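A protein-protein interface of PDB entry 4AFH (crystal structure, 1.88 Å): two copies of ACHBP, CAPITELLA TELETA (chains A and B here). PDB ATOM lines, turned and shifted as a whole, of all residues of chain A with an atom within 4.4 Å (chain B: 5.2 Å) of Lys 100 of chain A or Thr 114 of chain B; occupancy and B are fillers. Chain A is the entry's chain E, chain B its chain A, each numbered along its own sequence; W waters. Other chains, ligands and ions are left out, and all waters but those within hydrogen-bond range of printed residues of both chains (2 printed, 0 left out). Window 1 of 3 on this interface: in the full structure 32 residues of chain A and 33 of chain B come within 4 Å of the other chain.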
ATOM      1  N   ASP A  98      -9.648  -2.500  -2.269  1.00  0.00           N
ATOM      2  CA  ASP A  98     -10.994  -1.968  -2.420  1.00  0.00           C
ATOM      3  C   ASP A  98     -10.992  -0.521  -1.983  1.00  0.00           C
ATOM      4  O   ASP A  98     -11.786  -0.104  -1.133  1.00  0.00           O
ATOM      5  CB  ASP A  98     -11.989  -2.788  -1.595  1.00  0.00           C
ATOM      6  CG  ASP A  98     -11.678  -2.752  -0.117  1.00  0.00           C
ATOM      7  OD1 ASP A  98     -10.489  -2.559   0.247  1.00  0.00           O
ATOM      8  OD2 ASP A  98     -12.631  -2.894   0.675  1.00  0.00           O
ATOM      9  N   ILE A  99     -10.093   0.250  -2.575  1.00  0.00           N
ATOM     10  CA  ILE A  99      -9.983   1.663  -2.213  1.00  0.00           C
ATOM     11  C   ILE A  99     -11.063   2.500  -2.939  1.00  0.00           C
ATOM     12  O   ILE A  99     -11.169   2.486  -4.169  1.00  0.00           O
ATOM     13  CB  ILE A  99      -8.568   2.181  -2.442  1.00  0.00           C
ATOM     14  CG1 ILE A  99      -7.619   1.525  -1.409  1.00  0.00           C
ATOM     15  CG2 ILE A  99      -8.542   3.712  -2.308  1.00  0.00           C
ATOM     16  CD1 ILE A  99      -6.165   1.774  -1.664  1.00  0.00           C
ATOM     17  N   LYS A 100     -11.893   3.179  -2.150  1.00  0.00           N
ATOM     18  CA  LYS A 100     -13.026   3.920  -2.684  1.00  0.00           C
ATOM     19  C   LYS A 100     -12.927   5.400  -2.284  1.00  0.00           C
ATOM     20  O   LYS A 100     -12.251   5.756  -1.315  1.00  0.00           O
ATOM     21  CB  LYS A 100     -14.343   3.319  -2.157  1.00  0.00           C
ATOM     22  CG  LYS A 100     -14.493   1.804  -2.411  1.00  0.00           C
ATOM     23  CD  LYS A 100     -15.892   1.338  -1.994  1.00  0.00           C
ATOM     24  CE  LYS A 100     -16.473   0.373  -3.003  1.00  0.00           C
ATOM     25  NZ  LYS A 100     -16.799   1.042  -4.293  1.00  0.00           N
ATOM     26  N   LEU A 101     -13.606   6.241  -3.048  1.00  0.00           N
ATOM     27  CA  LEU A 101     -13.752   7.659  -2.716  1.00  0.00           C
ATOM     28  C   LEU A 101     -14.973   7.760  -1.816  1.00  0.00           C
ATOM     29  O   LEU A 101     -16.121   7.696  -2.265  1.00  0.00           O
ATOM     30  CB  LEU A 101     -13.926   8.476  -4.014  1.00  0.00           C
ATOM     31  CG  LEU A 101     -14.204   9.982  -3.880  1.00  0.00           C
ATOM     32  CD1 LEU A 101     -12.991  10.678  -3.290  1.00  0.00           C
ATOM     33  CD2 LEU A 101     -14.547  10.560  -5.264  1.00  0.00           C
ATOM     34  N   PHE A 102     -14.726   7.876  -0.514  1.00  0.00           N
ATOM     35  CA  PHE A 102     -15.782   7.822   0.493  1.00  0.00           C
ATOM     36  C   PHE A 102     -16.854   8.913   0.300  1.00  0.00           C
ATOM     37  O   PHE A 102     -18.057   8.659   0.449  1.00  0.00           O
ATOM     38  CB  PHE A 102     -15.100   7.900   1.869  1.00  0.00           C
ATOM     39  CG  PHE A 102     -16.040   7.888   3.068  1.00  0.00           C
ATOM     40  CD1 PHE A 102     -16.920   6.858   3.290  1.00  0.00           C
ATOM     41  CD2 PHE A 102     -15.973   8.908   4.013  1.00  0.00           C
ATOM     42  CE1 PHE A 102     -17.752   6.857   4.423  1.00  0.00           C
ATOM     43  CE2 PHE A 102     -16.795   8.907   5.134  1.00  0.00           C
ATOM     44  CZ  PHE A 102     -17.676   7.871   5.336  1.00  0.00           C
ATOM     45  N   ASP A 108     -19.325   5.781  -6.147  1.00  0.00           N
ATOM     46  CA  ASP A 108     -17.881   5.786  -5.942  1.00  0.00           C
ATOM     47  C   ASP A 108     -17.269   6.584  -7.089  1.00  0.00           C
ATOM     48  O   ASP A 108     -17.963   6.935  -8.043  1.00  0.00           O
ATOM     49  CB  ASP A 108     -17.361   4.322  -5.977  1.00  0.00           C
ATOM     50  CG  ASP A 108     -15.928   4.177  -5.457  1.00  0.00           C
ATOM     51  OD1 ASP A 108     -15.326   5.186  -5.019  1.00  0.00           O
ATOM     52  OD2 ASP A 108     -15.392   3.042  -5.480  1.00  0.00           O
ATOM     53  N   GLN A 149     -11.606  11.929   0.000  1.00  0.00           N
ATOM     54  CA  GLN A 149     -11.245  10.972   1.036  1.00  0.00           C
ATOM     55  C   GLN A 149     -11.190   9.579   0.459  1.00  0.00           C
ATOM     56  O   GLN A 149     -12.221   9.055  -0.013  1.00  0.00           O
ATOM     57  CB  GLN A 149     -12.286  11.007   2.157  1.00  0.00           C
ATOM     58  CG  GLN A 149     -12.421  12.360   2.811  1.00  0.00           C
ATOM     59  CD  GLN A 149     -13.691  12.473   3.611  1.00  0.00           C
ATOM     60  OE1 GLN A 149     -14.665  13.073   3.159  1.00  0.00           O
ATOM     61  NE2 GLN A 149     -13.693  11.890   4.805  1.00  0.00           N
ATOM     62  N   PHE A 150     -10.003   8.978   0.485  1.00  0.00           N
ATOM     63  CA  PHE A 150      -9.810   7.630  -0.042  1.00  0.00           C
ATOM     64  C   PHE A 150      -9.425   6.641   1.034  1.00  0.00           C
ATOM     65  O   PHE A 150      -8.646   6.960   1.929  1.00  0.00           O
ATOM     66  CB  PHE A 150      -8.692   7.600  -1.080  1.00  0.00           C
ATOM     67  CG  PHE A 150      -8.893   8.540  -2.226  1.00  0.00           C
ATOM     68  CD1 PHE A 150      -9.649   8.162  -3.335  1.00  0.00           C
ATOM     69  CD2 PHE A 150      -8.300   9.802  -2.211  1.00  0.00           C
ATOM     70  CE1 PHE A 150      -9.812   9.049  -4.417  1.00  0.00           C
ATOM     71  CE2 PHE A 150      -8.451  10.688  -3.273  1.00  0.00           C
ATOM     72  CZ  PHE A 150      -9.190  10.315  -4.379  1.00  0.00           C
ATOM     73  N   GLY A 151      -9.900   5.405   0.909  1.00  0.00           N
ATOM     74  CA  GLY A 151      -9.536   4.385   1.873  1.00  0.00           C
ATOM     75  C   GLY A 151     -10.073   3.031   1.469  1.00  0.00           C
ATOM     76  O   GLY A 151     -10.965   2.944   0.632  1.00  0.00           O
ATOM     77  N   TRP A 153     -12.448   0.047   1.755  1.00  0.00           N
ATOM     78  CA  TRP A 153     -13.795  -0.021   2.309  1.00  0.00           C
ATOM     79  C   TRP A 153     -13.912  -0.947   3.519  1.00  0.00           C
ATOM     80  O   TRP A 153     -14.510  -0.566   4.510  1.00  0.00           O
ATOM     81  CB  TRP A 153     -14.849  -0.405   1.257  1.00  0.00           C
ATOM     82  CG  TRP A 153     -16.231   0.024   1.687  1.00  0.00           C
ATOM     83  CD1 TRP A 153     -17.224  -0.766   2.164  1.00  0.00           C
ATOM     84  CD2 TRP A 153     -16.741   1.367   1.709  1.00  0.00           C
ATOM     85  NE1 TRP A 153     -18.340  -0.007   2.460  1.00  0.00           N
ATOM     86  CE2 TRP A 153     -18.061   1.306   2.197  1.00  0.00           C
ATOM     87  CE3 TRP A 153     -16.201   2.615   1.367  1.00  0.00           C
ATOM     88  CZ2 TRP A 153     -18.868   2.447   2.337  1.00  0.00           C
ATOM     89  CZ3 TRP A 153     -16.997   3.753   1.511  1.00  0.00           C
ATOM     90  CH2 TRP A 153     -18.310   3.659   1.986  1.00  0.00           C
ATOM     91  N   ASP B 112     -23.707  -0.064  -4.217  1.00  0.00           N
ATOM     92  CA  ASP B 112     -22.463  -0.506  -4.811  1.00  0.00           C
ATOM     93  C   ASP B 112     -22.246  -1.960  -4.417  1.00  0.00           C
ATOM     94  O   ASP B 112     -21.764  -2.246  -3.330  1.00  0.00           O
ATOM     95  CB  ASP B 112     -21.289   0.361  -4.356  1.00  0.00           C
ATOM     96  CG  ASP B 112     -20.017   0.080  -5.141  1.00  0.00           C
ATOM     97  OD1 ASP B 112     -19.912  -0.980  -5.804  1.00  0.00           O
ATOM     98  OD2 ASP B 112     -19.097   0.925  -5.082  1.00  0.00           O
ATOM     99  N   ARG B 113     -22.609  -2.871  -5.313  1.00  0.00           N
ATOM    100  CA  ARG B 113     -22.472  -4.295  -5.051  1.00  0.00           C
ATOM    101  C   ARG B 113     -21.055  -4.847  -5.321  1.00  0.00           C
ATOM    102  O   ARG B 113     -20.816  -6.039  -5.136  1.00  0.00           O
ATOM    103  CB  ARG B 113     -23.529  -5.092  -5.830  1.00  0.00           C
ATOM    104  CG  ARG B 113     -24.972  -4.580  -5.621  1.00  0.00           C
ATOM    105  CD  ARG B 113     -26.023  -5.535  -6.216  1.00  0.00           C
ATOM    106  NE  ARG B 113     -26.105  -6.773  -5.442  1.00  0.00           N
ATOM    107  CZ  ARG B 113     -26.962  -6.973  -4.442  1.00  0.00           C
ATOM    108  NH1 ARG B 113     -27.833  -6.032  -4.117  1.00  0.00           N
ATOM    109  NH2 ARG B 113     -26.960  -8.125  -3.779  1.00  0.00           N
ATOM    110  N   THR B 114     -20.118  -3.995  -5.737  1.00  0.00           N
ATOM    111  CA  THR B 114     -18.713  -4.420  -5.774  1.00  0.00           C
ATOM    112  C   THR B 114     -18.121  -4.378  -4.366  1.00  0.00           C
ATOM    113  O   THR B 114     -17.054  -4.932  -4.120  1.00  0.00           O
ATOM    114  CB  THR B 114     -17.834  -3.544  -6.676  1.00  0.00           C
ATOM    115  OG1 THR B 114     -17.658  -2.250  -6.073  1.00  0.00           O
ATOM    116  CG2 THR B 114     -18.446  -3.403  -8.084  1.00  0.00           C
ATOM    117  N   THR B 115     -18.822  -3.696  -3.461  1.00  0.00           N
ATOM    118  CA  THR B 115     -18.413  -3.589  -2.054  1.00  0.00           C
ATOM    119  C   THR B 115     -18.462  -4.973  -1.401  1.00  0.00           C
ATOM    120  O   THR B 115     -19.434  -5.697  -1.594  1.00  0.00           O
ATOM    121  CB  THR B 115     -19.353  -2.608  -1.319  1.00  0.00           C
ATOM    122  OG1 THR B 115     -19.226  -1.299  -1.910  1.00  0.00           O
ATOM    123  CG2 THR B 115     -19.030  -2.527   0.166  1.00  0.00           C
ATOM    124  N   GLN B 116     -17.425  -5.372  -0.662  1.00  0.00           N
ATOM    125  CA  GLN B 116     -17.462  -6.707  -0.035  1.00  0.00           C
ATOM    126  C   GLN B 116     -18.302  -6.751   1.238  1.00  0.00           C
ATOM    127  O   GLN B 116     -18.374  -5.771   1.969  1.00  0.00           O
ATOM    128  CB  GLN B 116     -16.054  -7.247   0.218  1.00  0.00           C
ATOM    129  CG  GLN B 116     -15.290  -7.439  -1.076  1.00  0.00           C
ATOM    130  CD  GLN B 116     -13.842  -7.780  -0.840  1.00  0.00           C
ATOM    131  OE1 GLN B 116     -13.040  -6.913  -0.482  1.00  0.00           O
ATOM    132  NE2 GLN B 116     -13.493  -9.050  -1.040  1.00  0.00           N
ATOM    133  N   PRO B 130     -22.194   1.734  -0.042  1.00  0.00           N
ATOM    134  CA  PRO B 130     -22.646   3.051  -0.487  1.00  0.00           C
ATOM    135  C   PRO B 130     -23.931   2.896  -1.320  1.00  0.00           C
ATOM    136  O   PRO B 130     -24.137   1.845  -1.938  1.00  0.00           O
ATOM    137  CB  PRO B 130     -21.520   3.522  -1.420  1.00  0.00           C
ATOM    138  CG  PRO B 130     -20.333   2.672  -1.095  1.00  0.00           C
ATOM    139  CD  PRO B 130     -20.905   1.350  -0.652  1.00  0.00           C
HETATM  140  O   HOH W   1     -16.797   0.823  -7.001  1.00  0.00           O
HETATM  141  O   HOH W   2     -14.873  -4.055  -0.460  1.00  0.00           O
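NZ of Lys 100 of chain A is in salt-bridge range of OD2 of Asp 112 of chain B (2.4 Å).
OD2 of Asp 108 of chain A lies within salt-bridge range of NZ of Lys 100 of chain A.
The side-chain carboxylate of Asp 108 of chain A is in hydrogen-bond range of the backbone NH of Leu 101 of chain A (2.8 Å).
N of Trp 153 of chain A sits at hydrogen-bond distance from O of Asp 98 of chain A.
OG1 of Thr 114 of chain B is in hydrogen-bond range of OD1 of Asp 112 of chain B (2.6 Å).
The backbone NH (N) of Asp 112 of chain B lies within hydrogen-bond range of the backbone carbonyl oxygen (O) of Pro 130 of chain B, at 3.0 Å.
O of Gly 151 of chain A lies within hydrogen-bond range of N of Lys 100 of chain A (2.9 Å).
NZ of Lys 100 of chain A touches OG1 of Thr 114 of chain B, at 3.8 Å.
Thr 115 of chain B touches Lys 100 of chain A (OG1 to CE, 3.4 Å).
Asp 108 of chain A touches Asp 112 of chain B (CB to OD2, 3.9 Å).
CG2 of Thr 115 of chain B touches CD1 of Trp 153 of chain A, at 3.2 Å.
Pro 130 of chain B touches Trp 153 of chain A (CG to CZ2, 3.7 Å).
Of the printed residues of chain B, Lys 100 of chain A touches Asp 112 (2.4 Å), Thr 114 (3.8 Å) and Thr 115 (3.4 Å).
Thr 114 of chain B touches just one residue of chain A: Lys 100 (3.8 Å).
Of the printed residues of chain B, Trp 153 of chain A touches Thr 115 (3.2 Å) and Pro 130 (3.7 Å).
Printed residues of chain A within 4 Å of Thr 115 of chain B: Lys 100 and Trp 153.
Of the printed residues of chain B, Asp 108 of chain A touches Asp 112 (3.9 Å).
Of the printed residues of chain A, Pro 130 of chain B touches Trp 153 (3.7 Å).
Of the printed residues of chain A, Asp 112 of chain B touches Lys 100 (2.4 Å) and Asp 108 (3.9 Å).
Asp 98 of chain A touches none of the printed residues of chain B.
The nearest printed residue of chain A that does not touch Thr 114 of chain B is Asp 108 of chain A (5.8 Å).
Of the 10 printed residues of chain A, 3 touch a printed residue of chain B.
Of the 6 printed residues of chain B, 4 touch a printed residue of chain A.
Hydrophobic or aromatic side chains of chain B within 4 Å of the printed part of chain A: Pro 130.
Among the printed residues, Asp or Glu carboxylates within 4 Å of a Lys or Arg side-chain nitrogen of the other chain: Lys 100 of chain A with Asp 112 of chain B.
No position is printed for both chains.
Of the 6 pairs that touch across the chains among the printed residues, none has its exchanged pair printed and touching as well.
Water W1 lies within hydrogen-bond range of the side-chain amino group (NZ) of Lys 100 of chain A (2.7 Å), the side-chain carboxylate (OD2) of Asp 112 of chain B (3.0 Å), the side-chain carboxylate (OD2) of Asp 108 of chain A (3.0 Å) and the side-chain hydroxyl (OG1) of Thr 114 of chain B (3.3 Å).
Water W2 bridges OD2 of Asp 98 of chain A (2.8 Å) and N of Gln 116 of chain B (2.9 Å).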
